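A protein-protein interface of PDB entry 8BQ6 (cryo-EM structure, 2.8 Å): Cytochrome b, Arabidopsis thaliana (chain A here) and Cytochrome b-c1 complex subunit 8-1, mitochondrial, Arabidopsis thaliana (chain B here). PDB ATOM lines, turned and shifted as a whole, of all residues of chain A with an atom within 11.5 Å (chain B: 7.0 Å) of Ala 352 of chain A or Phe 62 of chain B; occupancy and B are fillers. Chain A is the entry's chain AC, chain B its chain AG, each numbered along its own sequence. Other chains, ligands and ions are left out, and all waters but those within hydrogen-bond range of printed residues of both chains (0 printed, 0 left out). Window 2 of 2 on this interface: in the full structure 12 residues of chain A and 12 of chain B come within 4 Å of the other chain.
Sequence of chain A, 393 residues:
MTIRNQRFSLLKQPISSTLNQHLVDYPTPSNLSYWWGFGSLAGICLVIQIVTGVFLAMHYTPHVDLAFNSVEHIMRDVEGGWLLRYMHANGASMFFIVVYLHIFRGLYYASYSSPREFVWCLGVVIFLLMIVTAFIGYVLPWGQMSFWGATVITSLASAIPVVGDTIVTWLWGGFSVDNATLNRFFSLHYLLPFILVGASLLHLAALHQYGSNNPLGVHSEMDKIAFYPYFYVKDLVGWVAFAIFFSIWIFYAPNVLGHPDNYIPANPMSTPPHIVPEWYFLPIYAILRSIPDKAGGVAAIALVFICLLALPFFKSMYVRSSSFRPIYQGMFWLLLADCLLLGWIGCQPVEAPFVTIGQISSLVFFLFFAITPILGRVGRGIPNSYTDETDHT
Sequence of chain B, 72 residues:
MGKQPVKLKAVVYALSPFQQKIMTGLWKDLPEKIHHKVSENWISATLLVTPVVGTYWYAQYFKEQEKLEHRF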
ATOM      1  N   ARG A 289     -11.229 -27.061 -16.404  1.00  0.00           N
ATOM      2  CA  ARG A 289     -11.188 -26.518 -17.755  1.00  0.00           C
ATOM      3  C   ARG A 289     -11.003 -25.010 -17.785  1.00  0.00           C
ATOM      4  O   ARG A 289     -10.686 -24.465 -18.847  1.00  0.00           O
ATOM      5  CB  ARG A 289     -12.463 -26.882 -18.509  1.00  0.00           C
ATOM      6  CG  ARG A 289     -12.836 -28.336 -18.393  1.00  0.00           C
ATOM      7  CD  ARG A 289     -14.332 -28.477 -18.356  1.00  0.00           C
ATOM      8  NE  ARG A 289     -14.904 -28.671 -19.680  1.00  0.00           N
ATOM      9  CZ  ARG A 289     -16.204 -28.619 -19.937  1.00  0.00           C
ATOM     10  NH1 ARG A 289     -17.082 -28.329 -18.994  1.00  0.00           N
ATOM     11  NH2 ARG A 289     -16.638 -28.887 -21.161  1.00  0.00           N
ATOM     12  N   TRP A 344     -22.998 -25.506 -13.152  1.00  0.00           N
ATOM     13  CA  TRP A 344     -23.713 -25.295 -14.405  1.00  0.00           C
ATOM     14  C   TRP A 344     -22.746 -25.089 -15.565  1.00  0.00           C
ATOM     15  O   TRP A 344     -23.007 -25.538 -16.687  1.00  0.00           O
ATOM     16  CB  TRP A 344     -24.663 -24.105 -14.258  1.00  0.00           C
ATOM     17  CG  TRP A 344     -25.272 -23.626 -15.534  1.00  0.00           C
ATOM     18  CD1 TRP A 344     -26.225 -24.253 -16.279  1.00  0.00           C
ATOM     19  CD2 TRP A 344     -24.977 -22.400 -16.209  1.00  0.00           C
ATOM     20  NE1 TRP A 344     -26.537 -23.498 -17.382  1.00  0.00           N
ATOM     21  CE2 TRP A 344     -25.783 -22.353 -17.360  1.00  0.00           C
ATOM     22  CE3 TRP A 344     -24.107 -21.339 -15.952  1.00  0.00           C
ATOM     23  CZ2 TRP A 344     -25.745 -21.289 -18.252  1.00  0.00           C
ATOM     24  CZ3 TRP A 344     -24.070 -20.286 -16.838  1.00  0.00           C
ATOM     25  CH2 TRP A 344     -24.883 -20.266 -17.973  1.00  0.00           C
ATOM     26  N   ILE A 345     -21.622 -24.411 -15.315  1.00  0.00           N
ATOM     27  CA  ILE A 345     -20.640 -24.181 -16.371  1.00  0.00           C
ATOM     28  C   ILE A 345     -20.015 -25.497 -16.816  1.00  0.00           C
ATOM     29  O   ILE A 345     -19.831 -25.738 -18.016  1.00  0.00           O
ATOM     30  CB  ILE A 345     -19.572 -23.177 -15.899  1.00  0.00           C
ATOM     31  CG1 ILE A 345     -20.158 -21.768 -15.815  1.00  0.00           C
ATOM     32  CG2 ILE A 345     -18.377 -23.187 -16.834  1.00  0.00           C
ATOM     33  CD1 ILE A 345     -20.453 -21.155 -17.150  1.00  0.00           C
ATOM     34  N   GLN A 348     -21.714 -27.279 -19.635  1.00  0.00           N
ATOM     35  CA  GLN A 348     -21.778 -26.586 -20.911  1.00  0.00           C
ATOM     36  C   GLN A 348     -20.585 -26.943 -21.791  1.00  0.00           C
ATOM     37  O   GLN A 348     -19.519 -27.309 -21.286  1.00  0.00           O
ATOM     38  CB  GLN A 348     -21.810 -25.070 -20.694  1.00  0.00           C
ATOM     39  CG  GLN A 348     -22.981 -24.594 -19.862  1.00  0.00           C
ATOM     40  CD  GLN A 348     -24.304 -24.873 -20.534  1.00  0.00           C
ATOM     41  OE1 GLN A 348     -24.548 -24.424 -21.652  1.00  0.00           O
ATOM     42  NE2 GLN A 348     -25.167 -25.623 -19.860  1.00  0.00           N
ATOM     43  N   PRO A 349     -20.733 -26.854 -23.112  1.00  0.00           N
ATOM     44  CA  PRO A 349     -19.575 -27.045 -23.991  1.00  0.00           C
ATOM     45  C   PRO A 349     -18.574 -25.916 -23.826  1.00  0.00           C
ATOM     46  O   PRO A 349     -18.919 -24.795 -23.442  1.00  0.00           O
ATOM     47  CB  PRO A 349     -20.180 -27.053 -25.401  1.00  0.00           C
ATOM     48  CG  PRO A 349     -21.658 -27.072 -25.220  1.00  0.00           C
ATOM     49  CD  PRO A 349     -21.956 -26.541 -23.865  1.00  0.00           C
ATOM     50  N   VAL A 350     -17.317 -26.227 -24.125  1.00  0.00           N
ATOM     51  CA  VAL A 350     -16.229 -25.281 -23.923  1.00  0.00           C
ATOM     52  C   VAL A 350     -16.181 -24.299 -25.085  1.00  0.00           C
ATOM     53  O   VAL A 350     -15.491 -24.531 -26.086  1.00  0.00           O
ATOM     54  CB  VAL A 350     -14.885 -26.009 -23.764  1.00  0.00           C
ATOM     55  CG1 VAL A 350     -13.890 -25.127 -23.041  1.00  0.00           C
ATOM     56  CG2 VAL A 350     -15.079 -27.297 -23.026  1.00  0.00           C
ATOM     57  N   GLU A 351     -16.899 -23.191 -24.950  1.00  0.00           N
ATOM     58  CA  GLU A 351     -16.920 -22.154 -25.968  1.00  0.00           C
ATOM     59  C   GLU A 351     -17.434 -20.872 -25.331  1.00  0.00           C
ATOM     60  O   GLU A 351     -17.826 -20.851 -24.163  1.00  0.00           O
ATOM     61  CB  GLU A 351     -17.777 -22.566 -27.166  1.00  0.00           C
ATOM     62  CG  GLU A 351     -19.078 -23.234 -26.788  1.00  0.00           C
ATOM     63  CD  GLU A 351     -19.850 -23.684 -28.001  1.00  0.00           C
ATOM     64  OE1 GLU A 351     -21.063 -23.946 -27.875  1.00  0.00           O
ATOM     65  OE2 GLU A 351     -19.239 -23.776 -29.086  1.00  0.00           O
ATOM     66  N   ALA A 352     -17.415 -19.800 -26.113  1.00  0.00           N
ATOM     67  CA  ALA A 352     -17.873 -18.516 -25.613  1.00  0.00           C
ATOM     68  C   ALA A 352     -19.365 -18.582 -25.293  1.00  0.00           C
ATOM     69  O   ALA A 352     -20.135 -19.187 -26.043  1.00  0.00           O
ATOM     70  CB  ALA A 352     -17.607 -17.417 -26.639  1.00  0.00           C
ATOM     71  N   PRO A 353     -19.808 -17.959 -24.194  1.00  0.00           N
ATOM     72  CA  PRO A 353     -19.072 -17.147 -23.225  1.00  0.00           C
ATOM     73  C   PRO A 353     -18.659 -17.936 -21.990  1.00  0.00           C
ATOM     74  O   PRO A 353     -18.232 -17.367 -20.989  1.00  0.00           O
ATOM     75  CB  PRO A 353     -20.092 -16.063 -22.872  1.00  0.00           C
ATOM     76  CG  PRO A 353     -21.456 -16.745 -23.047  1.00  0.00           C
ATOM     77  CD  PRO A 353     -21.230 -18.027 -23.826  1.00  0.00           C
ATOM     78  N   PHE A 354     -18.789 -19.259 -22.033  1.00  0.00           N
ATOM     79  CA  PHE A 354     -18.594 -20.069 -20.840  1.00  0.00           C
ATOM     80  C   PHE A 354     -17.148 -20.128 -20.387  1.00  0.00           C
ATOM     81  O   PHE A 354     -16.897 -20.395 -19.206  1.00  0.00           O
ATOM     82  CB  PHE A 354     -19.122 -21.475 -21.091  1.00  0.00           C
ATOM     83  CG  PHE A 354     -20.551 -21.495 -21.500  1.00  0.00           C
ATOM     84  CD1 PHE A 354     -21.527 -21.018 -20.646  1.00  0.00           C
ATOM     85  CD2 PHE A 354     -20.919 -21.947 -22.750  1.00  0.00           C
ATOM     86  CE1 PHE A 354     -22.847 -21.019 -21.020  1.00  0.00           C
ATOM     87  CE2 PHE A 354     -22.241 -21.949 -23.129  1.00  0.00           C
ATOM     88  CZ  PHE A 354     -23.205 -21.482 -22.263  1.00  0.00           C
ATOM     89  N   VAL A 355     -16.191 -19.891 -21.282  1.00  0.00           N
ATOM     90  CA  VAL A 355     -14.797 -19.853 -20.859  1.00  0.00           C
ATOM     91  C   VAL A 355     -14.550 -18.647 -19.964  1.00  0.00           C
ATOM     92  O   VAL A 355     -13.936 -18.761 -18.897  1.00  0.00           O
ATOM     93  CB  VAL A 355     -13.856 -19.856 -22.074  1.00  0.00           C
ATOM     94  CG1 VAL A 355     -12.420 -19.768 -21.607  1.00  0.00           C
ATOM     95  CG2 VAL A 355     -14.062 -21.114 -22.894  1.00  0.00           C
ATOM     96  N   THR A 356     -15.026 -17.471 -20.384  1.00  0.00           N
ATOM     97  CA  THR A 356     -14.869 -16.280 -19.555  1.00  0.00           C
ATOM     98  C   THR A 356     -15.633 -16.418 -18.246  1.00  0.00           C
ATOM     99  O   THR A 356     -15.134 -16.032 -17.183  1.00  0.00           O
ATOM    100  CB  THR A 356     -15.340 -15.040 -20.314  1.00  0.00           C
ATOM    101  OG1 THR A 356     -14.688 -14.978 -21.587  1.00  0.00           O
ATOM    102  CG2 THR A 356     -15.009 -13.787 -19.528  1.00  0.00           C
ATOM    103  N   ILE A 357     -16.849 -16.965 -18.305  1.00  0.00           N
ATOM    104  CA  ILE A 357     -17.652 -17.131 -17.097  1.00  0.00           C
ATOM    105  C   ILE A 357     -17.037 -18.185 -16.184  1.00  0.00           C
ATOM    106  O   ILE A 357     -17.060 -18.052 -14.955  1.00  0.00           O
ATOM    107  CB  ILE A 357     -19.107 -17.468 -17.466  1.00  0.00           C
ATOM    108  CG1 ILE A 357     -19.743 -16.295 -18.208  1.00  0.00           C
ATOM    109  CG2 ILE A 357     -19.911 -17.781 -16.224  1.00  0.00           C
ATOM    110  CD1 ILE A 357     -21.089 -16.606 -18.796  1.00  0.00           C
ATOM    111  N   GLY A 358     -16.483 -19.250 -16.768  1.00  0.00           N
ATOM    112  CA  GLY A 358     -15.826 -20.262 -15.959  1.00  0.00           C
ATOM    113  C   GLY A 358     -14.580 -19.739 -15.269  1.00  0.00           C
ATOM    114  O   GLY A 358     -14.287 -20.109 -14.130  1.00  0.00           O
ATOM    115  N   GLN A 359     -13.831 -18.873 -15.953  1.00  0.00           N
ATOM    116  CA  GLN A 359     -12.609 -18.318 -15.379  1.00  0.00           C
ATOM    117  C   GLN A 359     -12.917 -17.346 -14.246  1.00  0.00           C
ATOM    118  O   GLN A 359     -12.180 -17.273 -13.256  1.00  0.00           O
ATOM    119  CB  GLN A 359     -11.793 -17.629 -16.472  1.00  0.00           C
ATOM    120  CG  GLN A 359     -10.699 -18.493 -17.063  1.00  0.00           C
ATOM    121  CD  GLN A 359     -10.464 -18.226 -18.534  1.00  0.00           C
ATOM    122  OE1 GLN A 359     -10.940 -17.236 -19.085  1.00  0.00           O
ATOM    123  NE2 GLN A 359      -9.712 -19.110 -19.177  1.00  0.00           N
ATOM    124  N   TYR B  56     -26.975 -16.568 -15.860  1.00  0.00           N
ATOM    125  CA  TYR B  56     -27.758 -17.387 -16.776  1.00  0.00           C
ATOM    126  C   TYR B  56     -28.403 -16.538 -17.865  1.00  0.00           C
ATOM    127  O   TYR B  56     -28.403 -16.914 -19.042  1.00  0.00           O
ATOM    128  CB  TYR B  56     -28.820 -18.153 -15.992  1.00  0.00           C
ATOM    129  CG  TYR B  56     -29.617 -19.125 -16.815  1.00  0.00           C
ATOM    130  CD1 TYR B  56     -29.162 -20.417 -17.026  1.00  0.00           C
ATOM    131  CD2 TYR B  56     -30.829 -18.755 -17.375  1.00  0.00           C
ATOM    132  CE1 TYR B  56     -29.888 -21.309 -17.770  1.00  0.00           C
ATOM    133  CE2 TYR B  56     -31.562 -19.640 -18.121  1.00  0.00           C
ATOM    134  CZ  TYR B  56     -31.086 -20.917 -18.319  1.00  0.00           C
ATOM    135  OH  TYR B  56     -31.816 -21.812 -19.067  1.00  0.00           O
ATOM    136  N   TRP B  57     -28.966 -15.386 -17.487  1.00  0.00           N
ATOM    137  CA  TRP B  57     -29.639 -14.537 -18.467  1.00  0.00           C
ATOM    138  C   TRP B  57     -28.661 -13.986 -19.490  1.00  0.00           C
ATOM    139  O   TRP B  57     -29.000 -13.841 -20.669  1.00  0.00           O
ATOM    140  CB  TRP B  57     -30.372 -13.393 -17.769  1.00  0.00           C
ATOM    141  CG  TRP B  57     -31.602 -12.968 -18.496  1.00  0.00           C
ATOM    142  CD1 TRP B  57     -31.711 -12.658 -19.821  1.00  0.00           C
ATOM    143  CD2 TRP B  57     -32.919 -12.864 -17.949  1.00  0.00           C
ATOM    144  NE1 TRP B  57     -33.011 -12.339 -20.125  1.00  0.00           N
ATOM    145  CE2 TRP B  57     -33.774 -12.462 -18.994  1.00  0.00           C
ATOM    146  CE3 TRP B  57     -33.457 -13.063 -16.675  1.00  0.00           C
ATOM    147  CZ2 TRP B  57     -35.138 -12.253 -18.802  1.00  0.00           C
ATOM    148  CZ3 TRP B  57     -34.810 -12.854 -16.487  1.00  0.00           C
ATOM    149  CH2 TRP B  57     -35.636 -12.455 -17.544  1.00  0.00           C
ATOM    150  N   TYR B  58     -27.452 -13.639 -19.053  1.00  0.00           N
ATOM    151  CA  TYR B  58     -26.455 -13.145 -19.992  1.00  0.00           C
ATOM    152  C   TYR B  58     -26.033 -14.235 -20.968  1.00  0.00           C
ATOM    153  O   TYR B  58     -25.810 -13.965 -22.153  1.00  0.00           O
ATOM    154  CB  TYR B  58     -25.248 -12.591 -19.236  1.00  0.00           C
ATOM    155  CG  TYR B  58     -24.057 -12.309 -20.119  1.00  0.00           C
ATOM    156  CD1 TYR B  58     -23.905 -11.075 -20.728  1.00  0.00           C
ATOM    157  CD2 TYR B  58     -23.076 -13.268 -20.326  1.00  0.00           C
ATOM    158  CE1 TYR B  58     -22.820 -10.810 -21.533  1.00  0.00           C
ATOM    159  CE2 TYR B  58     -21.988 -13.012 -21.131  1.00  0.00           C
ATOM    160  CZ  TYR B  58     -21.864 -11.779 -21.730  1.00  0.00           C
ATOM    161  OH  TYR B  58     -20.780 -11.513 -22.532  1.00  0.00           O
ATOM    162  N   ALA B  59     -25.902 -15.474 -20.485  1.00  0.00           N
ATOM    163  CA  ALA B  59     -25.469 -16.560 -21.358  1.00  0.00           C
ATOM    164  C   ALA B  59     -26.498 -16.842 -22.447  1.00  0.00           C
ATOM    165  O   ALA B  59     -26.133 -17.109 -23.597  1.00  0.00           O
ATOM    166  CB  ALA B  59     -25.190 -17.818 -20.538  1.00  0.00           C
ATOM    167  N   GLN B  60     -27.787 -16.799 -22.105  1.00  0.00           N
ATOM    168  CA  GLN B  60     -28.824 -16.923 -23.127  1.00  0.00           C
ATOM    169  C   GLN B  60     -28.827 -15.719 -24.057  1.00  0.00           C
ATOM    170  O   GLN B  60     -29.082 -15.848 -25.259  1.00  0.00           O
ATOM    171  CB  GLN B  60     -30.195 -17.094 -22.474  1.00  0.00           C
ATOM    172  CG  GLN B  60     -30.730 -18.520 -22.472  1.00  0.00           C
ATOM    173  CD  GLN B  60     -29.835 -19.497 -21.741  1.00  0.00           C
ATOM    174  OE1 GLN B  60     -29.437 -19.261 -20.602  1.00  0.00           O
ATOM    175  NE2 GLN B  60     -29.526 -20.613 -22.390  1.00  0.00           N
ATOM    176  N   TYR B  61     -28.568 -14.533 -23.511  1.00  0.00           N
ATOM    177  CA  TYR B  61     -28.474 -13.342 -24.343  1.00  0.00           C
ATOM    178  C   TYR B  61     -27.270 -13.412 -25.273  1.00  0.00           C
ATOM    179  O   TYR B  61     -27.335 -12.969 -26.423  1.00  0.00           O
ATOM    180  CB  TYR B  61     -28.405 -12.106 -23.454  1.00  0.00           C
ATOM    181  CG  TYR B  61     -27.941 -10.876 -24.173  1.00  0.00           C
ATOM    182  CD1 TYR B  61     -26.632 -10.439 -24.053  1.00  0.00           C
ATOM    183  CD2 TYR B  61     -28.809 -10.147 -24.967  1.00  0.00           C
ATOM    184  CE1 TYR B  61     -26.201  -9.316 -24.709  1.00  0.00           C
ATOM    185  CE2 TYR B  61     -28.389  -9.020 -25.622  1.00  0.00           C
ATOM    186  CZ  TYR B  61     -27.085  -8.607 -25.490  1.00  0.00           C
ATOM    187  OH  TYR B  61     -26.659  -7.479 -26.146  1.00  0.00           O
ATOM    188  N   PHE B  62     -26.149 -13.947 -24.787  1.00  0.00           N
ATOM    189  CA  PHE B  62     -24.981 -14.092 -25.651  1.00  0.00           C
ATOM    190  C   PHE B  62     -25.242 -15.097 -26.765  1.00  0.00           C
ATOM    191  O   PHE B  62     -24.995 -14.809 -27.943  1.00  0.00           O
ATOM    192  CB  PHE B  62     -23.765 -14.515 -24.830  1.00  0.00           C
ATOM    193  CG  PHE B  62     -22.488 -14.550 -25.618  1.00  0.00           C
ATOM    194  CD1 PHE B  62     -22.141 -15.676 -26.348  1.00  0.00           C
ATOM    195  CD2 PHE B  62     -21.632 -13.465 -25.623  1.00  0.00           C
ATOM    196  CE1 PHE B  62     -20.975 -15.711 -27.076  1.00  0.00           C
ATOM    197  CE2 PHE B  62     -20.458 -13.498 -26.347  1.00  0.00           C
ATOM    198  CZ  PHE B  62     -20.131 -14.623 -27.074  1.00  0.00           C
ATOM    199  N   LYS B  63     -25.749 -16.280 -26.409  1.00  0.00           N
ATOM    200  CA  LYS B  63     -25.943 -17.346 -27.387  1.00  0.00           C
ATOM    201  C   LYS B  63     -26.946 -16.953 -28.462  1.00  0.00           C
ATOM    202  O   LYS B  63     -26.812 -17.359 -29.621  1.00  0.00           O
ATOM    203  CB  LYS B  63     -26.409 -18.617 -26.688  1.00  0.00           C
ATOM    204  CG  LYS B  63     -25.406 -19.226 -25.734  1.00  0.00           C
ATOM    205  CD  LYS B  63     -25.363 -20.739 -25.881  1.00  0.00           C
ATOM    206  CE  LYS B  63     -26.735 -21.329 -26.199  1.00  0.00           C
ATOM    207  NZ  LYS B  63     -27.771 -20.991 -25.181  1.00  0.00           N
ATOM    208  N   GLU B  64     -27.984 -16.202 -28.089  1.00  0.00           N
ATOM    209  CA  GLU B  64     -28.959 -15.762 -29.080  1.00  0.00           C
ATOM    210  C   GLU B  64     -28.331 -14.822 -30.103  1.00  0.00           C
ATOM    211  O   GLU B  64     -28.521 -14.995 -31.312  1.00  0.00           O
ATOM    212  CB  GLU B  64     -30.146 -15.089 -28.398  1.00  0.00           C
ATOM    213  CG  GLU B  64     -31.290 -14.793 -29.350  1.00  0.00           C
ATOM    214  CD  GLU B  64     -32.197 -15.982 -29.613  1.00  0.00           C
ATOM    215  OE1 GLU B  64     -31.734 -17.004 -30.162  1.00  0.00           O
ATOM    216  OE2 GLU B  64     -33.399 -15.876 -29.297  1.00  0.00           O
ATOM    217  N   GLN B  65     -27.596 -13.804 -29.643  1.00  0.00           N
ATOM    218  CA  GLN B  65     -26.982 -12.886 -30.600  1.00  0.00           C
ATOM    219  C   GLN B  65     -25.959 -13.600 -31.469  1.00  0.00           C
ATOM    220  O   GLN B  65     -25.951 -13.424 -32.691  1.00  0.00           O
ATOM    221  CB  GLN B  65     -26.330 -11.695 -29.897  1.00  0.00           C
ATOM    222  CG  GLN B  65     -27.122 -11.105 -28.762  1.00  0.00           C
ATOM    223  CD  GLN B  65     -28.511 -10.679 -29.173  1.00  0.00           C
ATOM    224  OE1 GLN B  65     -28.707 -10.096 -30.236  1.00  0.00           O
ATOM    225  NE2 GLN B  65     -29.491 -10.983 -28.331  1.00  0.00           N
ATOM    226  N   GLU B  66     -25.103 -14.424 -30.863  1.00  0.00           N
ATOM    227  CA  GLU B  66     -24.089 -15.135 -31.635  1.00  0.00           C
ATOM    228  C   GLU B  66     -24.727 -16.053 -32.671  1.00  0.00           C
ATOM    229  O   GLU B  66     -24.150 -16.296 -33.737  1.00  0.00           O
ATOM    230  CB  GLU B  66     -23.179 -15.931 -30.696  1.00  0.00           C
ATOM    231  CG  GLU B  66     -23.467 -17.424 -30.680  1.00  0.00           C
ATOM    232  CD  GLU B  66     -22.464 -18.216 -29.873  1.00  0.00           C
ATOM    233  OE1 GLU B  66     -21.285 -17.809 -29.823  1.00  0.00           O
ATOM    234  OE2 GLU B  66     -22.862 -19.244 -29.283  1.00  0.00           O
ATOM    235  N   LYS B  67     -25.920 -16.572 -32.372  1.00  0.00           N
ATOM    236  CA  LYS B  67     -26.612 -17.441 -33.316  1.00  0.00           C
ATOM    237  C   LYS B  67     -27.188 -16.642 -34.474  1.00  0.00           C
ATOM    238  O   LYS B  67     -27.405 -17.177 -35.567  1.00  0.00           O
ATOM    239  CB  LYS B  67     -27.722 -18.206 -32.600  1.00  0.00           C
ATOM    240  CG  LYS B  67     -28.315 -19.336 -33.413  1.00  0.00           C
ATOM    241  CD  LYS B  67     -29.660 -19.756 -32.862  1.00  0.00           C
ATOM    242  CE  LYS B  67     -30.523 -18.539 -32.596  1.00  0.00           C
ATOM    243  NZ  LYS B  67     -31.875 -18.638 -33.206  1.00  0.00           N
ATOM    244  N   LEU B  68     -27.446 -15.356 -34.247  1.00  0.00           N
ATOM    245  CA  LEU B  68     -28.048 -14.524 -35.279  1.00  0.00           C
ATOM    246  C   LEU B  68     -26.996 -13.837 -36.138  1.00  0.00           C
ATOM    247  O   LEU B  68     -27.301 -13.407 -37.255  1.00  0.00           O
ATOM    248  CB  LEU B  68     -28.961 -13.492 -34.632  1.00  0.00           C
ATOM    249  CG  LEU B  68     -30.198 -13.998 -33.896  1.00  0.00           C
ATOM    250  CD1 LEU B  68     -30.932 -12.875 -33.179  1.00  0.00           C
ATOM    251  CD2 LEU B  68     -31.100 -14.649 -34.918  1.00  0.00           C
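The side-chain amide oxygen of Gln 60 of chain B lies close to the backbone carbonyl oxygen of Tyr 56 of chain B (3.0 Å).
CZ2 of Trp 344 of chain A touches CD1 of Tyr 56 of chain B, at 3.7 Å. CB of Ala 59 of chain B touches CH2 of Trp 344 of chain A, 3.6 Å away. Phe 62 of chain B touches Ala 352 of chain A (CE1 to O, 3.7 Å). Pro 353 of chain A touches Tyr 58 of chain B (CB to CE2, 3.99 Å). CG of Pro 353 of chain A touches CG of Phe 62 of chain B, 3.5 Å away. Phe 354 of chain A touches Ala 59 of chain B.
Printed residues of chain B within 4 Å of Trp 344 of chain A: Tyr 56 (3.7 Å) and Ala 59 (3.6 Å). Ala 352 of chain A touches just one residue of chain B: Phe 62. Of the printed residues of chain B, Pro 353 of chain A touches Tyr 58 and Phe 62. Printed residues of chain B within 4 Å of Phe 354 of chain A: Ala 59. Printed residues of chain A within 4 Å of Tyr 56 of chain B: Trp 344. Of chain A, only Ala 352 (3.7 Å) and Pro 353 (3.5 Å) come within 4 Å of Phe 62 of chain B. No residue of chain A comes within 4 Å of Gln 65 of chain B. Glu 66 of chain B touches none of the printed residues of chain A. Lys 67 of chain B touches none of the printed residues of chain A. Leu 68 of chain B touches none of the printed residues of chain A. The nearest residue of chain B that does not touch Ala 352 of chain A is Glu 66 of chain B (4.2 Å). The nearest residue of chain A that does not touch Phe 62 of chain B is Glu 351 of chain A (6.5 Å).
Printed residues of chain B that touch a printed residue of chain A: Tyr 56, Tyr 58, Ala 59 and Phe 62. Hydrophobic or aromatic side chains of chain B within 4 Å of the printed part of chain A: Tyr 56, Tyr 58, Ala 59 and Phe 62. Of the 15 printed residues of chain A, 4 touch a printed residue of chain B. Among the printed residues, 6 pairs touch across the chains. Among the printed residues, no Asp or Glu carboxylate lies within 4 Å of a Lys or Arg side-chain nitrogen of the other chain.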
